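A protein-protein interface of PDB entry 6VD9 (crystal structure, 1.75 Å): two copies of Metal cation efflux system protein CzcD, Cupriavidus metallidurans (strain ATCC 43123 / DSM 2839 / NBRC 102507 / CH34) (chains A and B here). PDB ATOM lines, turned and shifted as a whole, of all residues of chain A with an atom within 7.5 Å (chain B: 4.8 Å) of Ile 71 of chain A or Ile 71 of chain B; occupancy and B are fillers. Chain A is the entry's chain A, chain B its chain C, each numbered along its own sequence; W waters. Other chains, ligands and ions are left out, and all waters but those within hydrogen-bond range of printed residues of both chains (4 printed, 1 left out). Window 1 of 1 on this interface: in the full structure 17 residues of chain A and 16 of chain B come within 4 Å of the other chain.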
ATOM      1  N   ILE A  12     -13.855   7.976  11.819  1.00  0.00           N
ATOM      2  CA  ILE A  12     -13.840   8.605  10.469  1.00  0.00           C
ATOM      3  C   ILE A  12     -15.296   8.920  10.094  1.00  0.00           C
ATOM      4  O   ILE A  12     -15.592  10.098   9.826  1.00  0.00           O
ATOM      5  CB  ILE A  12     -13.136   7.716   9.421  1.00  0.00           C
ATOM      6  CG1 ILE A  12     -11.630   7.677   9.688  1.00  0.00           C
ATOM      7  CG2 ILE A  12     -13.434   8.190   8.019  1.00  0.00           C
ATOM      8  CD1 ILE A  12     -10.860   6.801   8.755  1.00  0.00           C
ATOM      9  N   LEU A  36      -1.072   6.084   7.763  1.00  0.00           N
ATOM     10  CA  LEU A  36      -2.488   5.847   7.382  1.00  0.00           C
ATOM     11  C   LEU A  36      -2.714   6.497   6.030  1.00  0.00           C
ATOM     12  O   LEU A  36      -2.294   7.646   5.860  1.00  0.00           O
ATOM     13  CB  LEU A  36      -3.418   6.457   8.426  1.00  0.00           C
ATOM     14  CG  LEU A  36      -4.922   6.330   8.154  1.00  0.00           C
ATOM     15  CD1 LEU A  36      -5.728   6.306   9.442  1.00  0.00           C
ATOM     16  CD2 LEU A  36      -5.417   7.466   7.281  1.00  0.00           C
ATOM     17  N   THR A  37      -3.406   5.803   5.131  1.00  0.00           N
ATOM     18  CA  THR A  37      -3.960   6.479   3.933  1.00  0.00           C
ATOM     19  C   THR A  37      -5.436   6.121   3.907  1.00  0.00           C
ATOM     20  O   THR A  37      -5.783   4.997   4.329  1.00  0.00           O
ATOM     21  CB  THR A  37      -3.234   6.117   2.634  1.00  0.00           C
ATOM     22  OG1 THR A  37      -3.417   4.725   2.423  1.00  0.00           O
ATOM     23  CG2 THR A  37      -1.743   6.394   2.698  1.00  0.00           C
ATOM     24  N   VAL A  38      -6.234   7.015   3.349  1.00  0.00           N
ATOM     25  CA  VAL A  38      -7.680   6.745   3.217  1.00  0.00           C
ATOM     26  C   VAL A  38      -8.253   7.641   2.132  1.00  0.00           C
ATOM     27  O   VAL A  38      -7.716   8.727   1.898  1.00  0.00           O
ATOM     28  CB  VAL A  38      -8.410   6.856   4.568  1.00  0.00           C
ATOM     29  CG1 VAL A  38      -8.445   8.273   5.119  1.00  0.00           C
ATOM     30  CG2 VAL A  38      -9.799   6.241   4.494  1.00  0.00           C
ATOM     31  N   HIS A  39      -9.260   7.125   1.427  1.00  0.00           N
ATOM     32  CA  HIS A  39     -10.090   7.904   0.475  1.00  0.00           C
ATOM     33  C   HIS A  39     -11.449   8.237   1.110  1.00  0.00           C
ATOM     34  O   HIS A  39     -12.215   7.318   1.418  1.00  0.00           O
ATOM     35  CB  HIS A  39     -10.215   7.201  -0.870  1.00  0.00           C
ATOM     36  CG  HIS A  39      -8.919   7.059  -1.590  1.00  0.00           C
ATOM     37  ND1 HIS A  39      -8.819   7.257  -2.949  1.00  0.00           N
ATOM     38  CD2 HIS A  39      -7.686   6.682  -1.178  1.00  0.00           C
ATOM     39  CE1 HIS A  39      -7.576   7.025  -3.331  1.00  0.00           C
ATOM     40  NE2 HIS A  39      -6.865   6.688  -2.272  1.00  0.00           N
ATOM     41  N   VAL A  40     -11.752   9.514   1.269  1.00  0.00           N
ATOM     42  CA  VAL A  40     -12.999   9.957   1.955  1.00  0.00           C
ATOM     43  C   VAL A  40     -13.947  10.558   0.923  1.00  0.00           C
ATOM     44  O   VAL A  40     -13.520  11.439   0.114  1.00  0.00           O
ATOM     45  CB  VAL A  40     -12.701  10.941   3.092  1.00  0.00           C
ATOM     46  CG1 VAL A  40     -13.964  11.576   3.629  1.00  0.00           C
ATOM     47  CG2 VAL A  40     -11.912  10.244   4.196  1.00  0.00           C
ATOM     48  N   PRO A  48     -13.866  19.983   2.033  1.00  0.00           N
ATOM     49  CA  PRO A  48     -13.228  19.151   3.065  1.00  0.00           C
ATOM     50  C   PRO A  48     -11.813  19.625   3.385  1.00  0.00           C
ATOM     51  O   PRO A  48     -11.366  19.357   4.468  1.00  0.00           O
ATOM     52  CB  PRO A  48     -13.213  17.722   2.489  1.00  0.00           C
ATOM     53  CG  PRO A  48     -13.235  17.989   0.966  1.00  0.00           C
ATOM     54  CD  PRO A  48     -14.076  19.241   0.784  1.00  0.00           C
ATOM     55  N   VAL A  52     -13.149  19.473   6.965  1.00  0.00           N
ATOM     56  CA  VAL A  52     -13.056  18.051   7.360  1.00  0.00           C
ATOM     57  C   VAL A  52     -11.591  17.701   7.642  1.00  0.00           C
ATOM     58  O   VAL A  52     -11.350  17.022   8.640  1.00  0.00           O
ATOM     59  CB  VAL A  52     -13.674  17.146   6.285  1.00  0.00           C
ATOM     60  CG1 VAL A  52     -13.632  15.712   6.741  1.00  0.00           C
ATOM     61  CG2 VAL A  52     -15.127  17.538   6.002  1.00  0.00           C
ATOM     62  N   LEU A  53     -10.646  18.075   6.765  1.00  0.00           N
ATOM     63  CA  LEU A  53      -9.232  17.597   6.917  1.00  0.00           C
ATOM     64  C   LEU A  53      -8.667  17.940   8.299  1.00  0.00           C
ATOM     65  O   LEU A  53      -8.039  17.102   8.938  1.00  0.00           O
ATOM     66  CB  LEU A  53      -8.382  18.147   5.780  1.00  0.00           C
ATOM     67  CG  LEU A  53      -6.908  17.737   5.781  1.00  0.00           C
ATOM     68  CD1 LEU A  53      -6.767  16.222   5.776  1.00  0.00           C
ATOM     69  CD2 LEU A  53      -6.221  18.293   4.581  1.00  0.00           C
ATOM     70  N   PRO A  54      -8.824  19.176   8.813  1.00  0.00           N
ATOM     71  CA  PRO A  54      -8.232  19.517  10.104  1.00  0.00           C
ATOM     72  C   PRO A  54      -8.822  18.674  11.239  1.00  0.00           C
ATOM     73  O   PRO A  54      -8.063  18.251  12.113  1.00  0.00           O
ATOM     74  CB  PRO A  54      -8.561  21.012  10.296  1.00  0.00           C
ATOM     75  CG  PRO A  54      -8.919  21.509   8.926  1.00  0.00           C
ATOM     76  CD  PRO A  54      -9.489  20.316   8.176  1.00  0.00           C
ATOM     77  N   GLU A  55     -10.133  18.386  11.176  1.00  0.00           N
ATOM     78  CA  GLU A  55     -10.829  17.544  12.185  1.00  0.00           C
ATOM     79  C   GLU A  55     -10.332  16.101  12.107  1.00  0.00           C
ATOM     80  O   GLU A  55     -10.105  15.499  13.159  1.00  0.00           O
ATOM     81  CB  GLU A  55     -12.343  17.604  12.005  1.00  0.00           C
ATOM     82  CG  GLU A  55     -12.893  18.989  12.288  1.00  0.00           C
ATOM     83  CD  GLU A  55     -12.798  20.091  11.240  1.00  0.00           C
ATOM     84  OE1 GLU A  55     -12.194  19.898  10.140  1.00  0.00           O
ATOM     85  OE2 GLU A  55     -13.339  21.209  11.547  1.00  0.00           O
ATOM     86  N   LEU A  56     -10.177  15.532  10.903  1.00  0.00           N
ATOM     87  CA  LEU A  56      -9.630  14.157  10.786  1.00  0.00           C
ATOM     88  C   LEU A  56      -8.183  14.123  11.306  1.00  0.00           C
ATOM     89  O   LEU A  56      -7.858  13.165  11.979  1.00  0.00           O
ATOM     90  CB  LEU A  56      -9.710  13.671   9.343  1.00  0.00           C
ATOM     91  CG  LEU A  56     -11.118  13.385   8.816  1.00  0.00           C
ATOM     92  CD1 LEU A  56     -11.066  13.080   7.326  1.00  0.00           C
ATOM     93  CD2 LEU A  56     -11.730  12.199   9.532  1.00  0.00           C
ATOM     94  N   LYS A  57      -7.349  15.076  10.941  1.00  0.00           N
ATOM     95  CA  LYS A  57      -5.937  15.125  11.425  1.00  0.00           C
ATOM     96  C   LYS A  57      -5.956  15.142  12.965  1.00  0.00           C
ATOM     97  O   LYS A  57      -5.213  14.356  13.568  1.00  0.00           O
ATOM     98  CB  LYS A  57      -5.182  16.329  10.864  1.00  0.00           C
ATOM     99  CG  LYS A  57      -4.789  16.241   9.380  1.00  0.00           C
ATOM    100  CD  LYS A  57      -4.303  17.581   8.865  1.00  0.00           C
ATOM    101  CE  LYS A  57      -3.668  17.561   7.493  1.00  0.00           C
ATOM    102  NZ  LYS A  57      -3.203  18.920   7.084  1.00  0.00           N
ATOM    103  N   MET A  59      -8.289  14.267  15.191  1.00  0.00           N
ATOM    104  CA  MET A  59      -8.872  13.046  15.792  1.00  0.00           C
ATOM    105  C   MET A  59      -7.861  11.903  15.672  1.00  0.00           C
ATOM    106  O   MET A  59      -7.731  11.092  16.617  1.00  0.00           O
ATOM    107  CB  MET A  59     -10.214  12.712  15.124  1.00  0.00           C
ATOM    108  CG  MET A  59     -10.756  11.363  15.510  1.00  0.00           C
ATOM    109  SD  MET A  59     -10.100  10.034  14.516  1.00  0.00           S
ATOM    110  CE  MET A  59     -10.827  10.393  12.910  1.00  0.00           C
ATOM    111  N   LEU A  60      -7.149  11.786  14.544  1.00  0.00           N
ATOM    112  CA  LEU A  60      -6.256  10.622  14.316  1.00  0.00           C
ATOM    113  C   LEU A  60      -5.039  10.726  15.246  1.00  0.00           C
ATOM    114  O   LEU A  60      -4.586   9.690  15.759  1.00  0.00           O
ATOM    115  CB  LEU A  60      -5.861  10.579  12.843  1.00  0.00           C
ATOM    116  CG  LEU A  60      -7.005  10.181  11.912  1.00  0.00           C
ATOM    117  CD1 LEU A  60      -6.612  10.447  10.469  1.00  0.00           C
ATOM    118  CD2 LEU A  60      -7.384   8.719  12.136  1.00  0.00           C
ATOM    119  N   VAL A  69      -0.233  10.881   7.932  1.00  0.00           N
ATOM    120  CA  VAL A  69      -1.576  10.732   7.300  1.00  0.00           C
ATOM    121  C   VAL A  69      -1.587  11.288   5.873  1.00  0.00           C
ATOM    122  O   VAL A  69      -1.017  12.357   5.613  1.00  0.00           O
ATOM    123  CB  VAL A  69      -2.610  11.420   8.203  1.00  0.00           C
ATOM    124  CG1 VAL A  69      -3.946  11.646   7.536  1.00  0.00           C
ATOM    125  CG2 VAL A  69      -2.786  10.657   9.502  1.00  0.00           C
ATOM    126  N   THR A  70      -2.305  10.606   4.983  1.00  0.00           N
ATOM    127  CA  THR A  70      -2.615  11.134   3.629  1.00  0.00           C
ATOM    128  C   THR A  70      -4.075  10.803   3.377  1.00  0.00           C
ATOM    129  O   THR A  70      -4.427   9.605   3.335  1.00  0.00           O
ATOM    130  CB  THR A  70      -1.701  10.583   2.527  1.00  0.00           C
ATOM    131  OG1 THR A  70      -0.349  10.731   2.973  1.00  0.00           O
ATOM    132  CG2 THR A  70      -1.871  11.320   1.217  1.00  0.00           C
ATOM    133  N   ILE A  71      -4.884  11.829   3.312  1.00  0.00           N
ATOM    134  CA  ILE A  71      -6.356  11.720   3.187  1.00  0.00           C
ATOM    135  C   ILE A  71      -6.740  12.358   1.855  1.00  0.00           C
ATOM    136  O   ILE A  71      -6.464  13.572   1.672  1.00  0.00           O
ATOM    137  CB  ILE A  71      -7.080  12.361   4.372  1.00  0.00           C
ATOM    138  CG1 ILE A  71      -6.706  11.643   5.665  1.00  0.00           C
ATOM    139  CG2 ILE A  71      -8.591  12.392   4.099  1.00  0.00           C
ATOM    140  CD1 ILE A  71      -7.055  12.402   6.941  1.00  0.00           C
ATOM    141  N   GLN A  72      -7.329  11.579   0.953  1.00  0.00           N
ATOM    142  CA  GLN A  72      -7.855  12.105  -0.327  1.00  0.00           C
ATOM    143  C   GLN A  72      -9.372  12.221  -0.234  1.00  0.00           C
ATOM    144  O   GLN A  72      -9.984  11.336   0.309  1.00  0.00           O
ATOM    145  CB  GLN A  72      -7.432  11.193  -1.472  1.00  0.00           C
ATOM    146  CG  GLN A  72      -7.981  11.558  -2.837  1.00  0.00           C
ATOM    147  CD  GLN A  72      -7.392  10.636  -3.893  1.00  0.00           C
ATOM    148  OE1 GLN A  72      -6.184  10.480  -3.996  1.00  0.00           O
ATOM    149  NE2 GLN A  72      -8.215   9.988  -4.707  1.00  0.00           N
ATOM    150  N   PHE A  73      -9.926  13.321  -0.721  1.00  0.00           N
ATOM    151  CA  PHE A  73     -11.393  13.519  -0.778  1.00  0.00           C
ATOM    152  C   PHE A  73     -11.916  13.391  -2.209  1.00  0.00           C
ATOM    153  O   PHE A  73     -11.296  13.971  -3.143  1.00  0.00           O
ATOM    154  CB  PHE A  73     -11.732  14.872  -0.191  1.00  0.00           C
ATOM    155  CG  PHE A  73     -11.337  15.047   1.243  1.00  0.00           C
ATOM    156  CD1 PHE A  73     -12.065  14.427   2.249  1.00  0.00           C
ATOM    157  CD2 PHE A  73     -10.299  15.906   1.603  1.00  0.00           C
ATOM    158  CE1 PHE A  73     -11.766  14.687   3.574  1.00  0.00           C
ATOM    159  CE2 PHE A  73      -9.965  16.107   2.929  1.00  0.00           C
ATOM    160  CZ  PHE A  73     -10.687  15.468   3.917  1.00  0.00           C
ATOM    161  N   VAL B  38       1.151  11.687  -1.680  1.00  0.00           N
ATOM    162  CA  VAL B  38       1.771  13.030  -1.746  1.00  0.00           C
ATOM    163  C   VAL B  38       0.825  14.041  -1.118  1.00  0.00           C
ATOM    164  O   VAL B  38      -0.401  13.829  -1.105  1.00  0.00           O
ATOM    165  CB  VAL B  38       2.121  13.420  -3.196  1.00  0.00           C
ATOM    166  CG1 VAL B  38       0.879  13.566  -4.079  1.00  0.00           C
ATOM    167  CG2 VAL B  38       2.950  14.683  -3.270  1.00  0.00           C
ATOM    168  N   VAL B  40      -0.162  17.961  -1.515  1.00  0.00           N
ATOM    169  CA  VAL B  40      -0.061  19.056  -2.504  1.00  0.00           C
ATOM    170  C   VAL B  40      -0.619  20.321  -1.844  1.00  0.00           C
ATOM    171  O   VAL B  40      -1.739  20.281  -1.304  1.00  0.00           O
ATOM    172  CB  VAL B  40      -0.781  18.652  -3.803  1.00  0.00           C
ATOM    173  CG1 VAL B  40      -0.927  19.814  -4.775  1.00  0.00           C
ATOM    174  CG2 VAL B  40      -0.081  17.483  -4.473  1.00  0.00           C
ATOM    175  N   LEU B  53      -7.408  17.303  -8.865  1.00  0.00           N
ATOM    176  CA  LEU B  53      -7.289  15.872  -8.505  1.00  0.00           C
ATOM    177  C   LEU B  53      -7.426  15.000  -9.750  1.00  0.00           C
ATOM    178  O   LEU B  53      -6.554  14.162 -10.007  1.00  0.00           O
ATOM    179  CB  LEU B  53      -8.287  15.517  -7.405  1.00  0.00           C
ATOM    180  CG  LEU B  53      -8.289  14.053  -6.995  1.00  0.00           C
ATOM    181  CD1 LEU B  53      -6.901  13.567  -6.582  1.00  0.00           C
ATOM    182  CD2 LEU B  53      -9.271  13.836  -5.870  1.00  0.00           C
ATOM    183  N   LEU B  56      -4.271  15.309 -11.913  1.00  0.00           N
ATOM    184  CA  LEU B  56      -3.078  14.606 -11.354  1.00  0.00           C
ATOM    185  C   LEU B  56      -3.208  13.088 -11.540  1.00  0.00           C
ATOM    186  O   LEU B  56      -2.200  12.423 -11.894  1.00  0.00           O
ATOM    187  CB  LEU B  56      -2.901  14.940  -9.867  1.00  0.00           C
ATOM    188  CG  LEU B  56      -2.348  16.322  -9.581  1.00  0.00           C
ATOM    189  CD1 LEU B  56      -2.537  16.704  -8.127  1.00  0.00           C
ATOM    190  CD2 LEU B  56      -0.895  16.404  -9.979  1.00  0.00           C
ATOM    191  N   LYS B  57      -4.390  12.532 -11.299  1.00  0.00           N
ATOM    192  CA  LYS B  57      -4.616  11.064 -11.420  1.00  0.00           C
ATOM    193  C   LYS B  57      -4.388  10.653 -12.883  1.00  0.00           C
ATOM    194  O   LYS B  57      -3.680   9.653 -13.118  1.00  0.00           O
ATOM    195  CB  LYS B  57      -6.028  10.697 -10.964  1.00  0.00           C
ATOM    196  CG  LYS B  57      -6.295  10.960  -9.492  1.00  0.00           C
ATOM    197  CD  LYS B  57      -7.723  10.727  -9.137  1.00  0.00           C
ATOM    198  CE  LYS B  57      -7.926  10.117  -7.766  1.00  0.00           C
ATOM    199  NZ  LYS B  57      -9.150   9.277  -7.709  1.00  0.00           N
ATOM    200  N   LEU B  60      -0.550  10.838 -13.680  1.00  0.00           N
ATOM    201  CA  LEU B  60       0.266   9.797 -13.023  1.00  0.00           C
ATOM    202  C   LEU B  60       0.009   8.474 -13.752  1.00  0.00           C
ATOM    203  O   LEU B  60       0.943   7.717 -13.932  1.00  0.00           O
ATOM    204  CB  LEU B  60      -0.054   9.721 -11.523  1.00  0.00           C
ATOM    205  CG  LEU B  60       0.411  10.918 -10.688  1.00  0.00           C
ATOM    206  CD1 LEU B  60      -0.147  10.853  -9.279  1.00  0.00           C
ATOM    207  CD2 LEU B  60       1.930  10.993 -10.636  1.00  0.00           C
ATOM    208  N   VAL B  69      -3.120   5.660  -5.906  1.00  0.00           N
ATOM    209  CA  VAL B  69      -2.685   7.020  -5.538  1.00  0.00           C
ATOM    210  C   VAL B  69      -3.513   7.503  -4.357  1.00  0.00           C
ATOM    211  O   VAL B  69      -4.715   7.225  -4.316  1.00  0.00           O
ATOM    212  CB  VAL B  69      -2.859   7.946  -6.752  1.00  0.00           C
ATOM    213  CG1 VAL B  69      -2.756   9.404  -6.369  1.00  0.00           C
ATOM    214  CG2 VAL B  69      -1.873   7.591  -7.862  1.00  0.00           C
ATOM    215  N   THR B  70      -2.879   8.275  -3.480  1.00  0.00           N
ATOM    216  CA  THR B  70      -3.611   9.033  -2.453  1.00  0.00           C
ATOM    217  C   THR B  70      -2.971  10.411  -2.407  1.00  0.00           C
ATOM    218  O   THR B  70      -1.775  10.513  -2.141  1.00  0.00           O
ATOM    219  CB  THR B  70      -3.583   8.334  -1.091  1.00  0.00           C
ATOM    220  OG1 THR B  70      -3.953   6.950  -1.142  1.00  0.00           O
ATOM    221  CG2 THR B  70      -4.479   9.068  -0.112  1.00  0.00           C
ATOM    222  N   ILE B  71      -3.758  11.420  -2.748  1.00  0.00           N
ATOM    223  CA  ILE B  71      -3.311  12.827  -2.833  1.00  0.00           C
ATOM    224  C   ILE B  71      -4.105  13.671  -1.833  1.00  0.00           C
ATOM    225  O   ILE B  71      -5.357  13.805  -1.971  1.00  0.00           O
ATOM    226  CB  ILE B  71      -3.489  13.339  -4.266  1.00  0.00           C
ATOM    227  CG1 ILE B  71      -2.641  12.576  -5.284  1.00  0.00           C
ATOM    228  CG2 ILE B  71      -3.225  14.818  -4.319  1.00  0.00           C
ATOM    229  CD1 ILE B  71      -3.117  12.739  -6.717  1.00  0.00           C
ATOM    230  N   GLN B  72      -3.399  14.286  -0.886  1.00  0.00           N
ATOM    231  CA  GLN B  72      -3.987  15.179   0.113  1.00  0.00           C
ATOM    232  C   GLN B  72      -3.687  16.619  -0.296  1.00  0.00           C
ATOM    233  O   GLN B  72      -2.498  16.938  -0.536  1.00  0.00           O
ATOM    234  CB  GLN B  72      -3.409  14.876   1.483  1.00  0.00           C
ATOM    235  CG  GLN B  72      -3.889  15.814   2.574  1.00  0.00           C
ATOM    236  CD  GLN B  72      -3.432  15.314   3.916  1.00  0.00           C
ATOM    237  OE1 GLN B  72      -3.745  14.189   4.302  1.00  0.00           O
ATOM    238  NE2 GLN B  72      -2.709  16.162   4.632  1.00  0.00           N
ATOM    239  N   PHE B  73      -4.713  17.461  -0.345  1.00  0.00           N
ATOM    240  CA  PHE B  73      -4.559  18.902  -0.664  1.00  0.00           C
ATOM    241  C   PHE B  73      -4.620  19.690   0.631  1.00  0.00           C
ATOM    242  O   PHE B  73      -5.486  19.377   1.488  1.00  0.00           O
ATOM    243  CB  PHE B  73      -5.647  19.398  -1.595  1.00  0.00           C
ATOM    244  CG  PHE B  73      -5.565  18.770  -2.957  1.00  0.00           C
ATOM    245  CD1 PHE B  73      -4.541  19.109  -3.847  1.00  0.00           C
ATOM    246  CD2 PHE B  73      -6.503  17.844  -3.345  1.00  0.00           C
ATOM    247  CE1 PHE B  73      -4.464  18.526  -5.101  1.00  0.00           C
ATOM    248  CE2 PHE B  73      -6.446  17.282  -4.612  1.00  0.00           C
ATOM    249  CZ  PHE B  73      -5.411  17.598  -5.476  1.00  0.00           C
HETATM  250  O   HOH W   1      -1.332  15.129   7.183  1.00  0.00           O
HETATM  251  O   HOH W   2      -7.149  15.985   0.585  1.00  0.00           O
HETATM  252  O   HOH W   3      -7.782  15.024  -1.793  1.00  0.00           O
HETATM  253  O   HOH W   4      -5.465   4.479   0.739  1.00  0.00           O
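A ring nitrogen (NE2) of His 39 of chain A is in hydrogen-bond range of the backbone carbonyl oxygen (O) of Val 69 of chain B, at 3.0 Å. NE2 of His 39 of chain A is in hydrogen-bond range of OG1 of Thr 70 of chain B, 3.1 Å away. OE1 of Gln 72 of chain B sits at hydrogen-bond distance from N of Ile 71 of chain A. The side-chain amino group (NZ) of Lys 57 of chain B sits close to the side-chain amide nitrogen (NE2) of Gln 72 of chain A, 3.2 Å away. The side-chain amide oxygen (OE1) of Gln 72 of chain A is in hydrogen-bond range of the backbone NH (N) of Ile 71 of chain B (2.9 Å).
O of Thr 70 of chain A is in hydrogen-bond range of N of Val 38 of chain A (3.2 Å). ND1 of His 39 of chain A lies within hydrogen-bond range of NE2 of Gln 72 of chain A (3.3 Å). N of Leu 53 of chain A lies within hydrogen-bond range of O of Pro 48 of chain A, 2.7 Å away. The backbone NH of Val 38 of chain B sits at hydrogen-bond distance from the backbone carbonyl oxygen of Thr 70 of chain B, 3.2 Å away. N of Gln 72 of chain B sits at hydrogen-bond distance from O of Val 38 of chain B (3.0 Å). The backbone carbonyl oxygen of Gln 72 of chain B lies within hydrogen-bond range of the backbone NH of Val 40 of chain B (2.7 Å).
CB of Thr 37 of chain A touches OG1 of Thr 70 of chain B (3.9 Å). Thr 70 of chain B touches Val 38 of chain A (CG2 to O, 3.8 Å). CD1 of Leu 53 of chain A touches CD of Gln 72 of chain B, at 3.9 Å. Leu 53 of chain A touches Phe 73 of chain B. Lys 57 of chain A touches Gln 72 of chain B. Val 69 of chain A touches Gln 72 of chain B (O to OE1, 3.5 Å). Thr 70 of chain A touches Thr 70 of chain B (CG2 to O, 3.5 Å). CA of Thr 70 of chain A touches OE1 of Gln 72 of chain B, at 3.3 Å. OE1 of Gln 72 of chain A touches O of Val 69 of chain B, at 3.6 Å. Gln 72 of chain A touches Thr 70 of chain B (OE1 to CA, 3.3 Å).
Printed residues of chain B within 4 Å of Thr 37 of chain A: Thr 70. Printed residues of chain B within 4 Å of Val 38 of chain A: Thr 70. Pro 48 of chain A touches none of the printed residues of chain B. Of the printed residues of chain B, Val 69 of chain A touches Gln 72. Ile 71 of chain A touches just these residues of chain B: Ile 71 and Gln 72. Leu 60 of chain B touches none of the printed residues of chain A. Of the printed residues of chain A, Ile 71 of chain B touches Ile 71 (3.8 Å) and Gln 72 (2.9 Å). The nearest residue of chain B that does not touch Ile 71 of chain A is Thr 70 of chain B (4.4 Å). The nearest residue of chain A that does not touch Ile 71 of chain B is Thr 70 of chain A (4.4 Å). The nearest printed residue of chain B that does not touch Lys 57 of chain A is Phe 73 of chain B (6.1 Å).
Hydrophobic or aromatic side chains of chain A within 4 Å of the printed part of chain B: His 39, Leu 53 and Ile 71. Of the 11 printed residues of chain B, 8 touch a printed residue of chain A. Hydrophobic or aromatic side chains of chain B within 4 Å of the printed part of chain A: Leu 53 and Ile 71. Among the printed residues, 18 pairs touch across the chains. Among the printed residues, no Asp or Glu carboxylate lies within 4 Å of a Lys or Arg side-chain nitrogen of the other chain.
Lys 57 of chain A touches Gln 72 of chain B, and with the chains exchanged Gln 72 of chain A touches Lys 57 of chain B. Thr 70 of chain A touches its own counterpart, Thr 70 of chain B. Thr 70 of chain A touches Gln 72 of chain B, and with the chains exchanged Gln 72 of chain A touches Thr 70 of chain B. Ile 71 of chain A touches Gln 72 of chain B, and with the chains exchanged Gln 72 of chain A touches Ile 71 of chain B. Of the 18 pairs that touch across the chains among the printed residues, 14 have their exchanged pair printed and touching as well.
Water W4 bridges OG1 of Thr 37 of chain A (2.7 Å) and OG1 of Thr 70 of chain B (3.5 Å). Water W3 bridges the backbone carbonyl oxygen (O) of Ile 71 of chain B (2.7 Å) and the backbone NH (N) of Phe 73 of chain A (2.9 Å). Water W2 lies within hydrogen-bond range of the backbone carbonyl oxygen of Ile 71 of chain A (2.7 Å) and the backbone NH of Phe 73 of chain B (3.0 Å). Water W1 bridges the side-chain amide nitrogen (NE2) of Gln 72 of chain B and the backbone carbonyl oxygen (O) of Val 69 of chain A.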
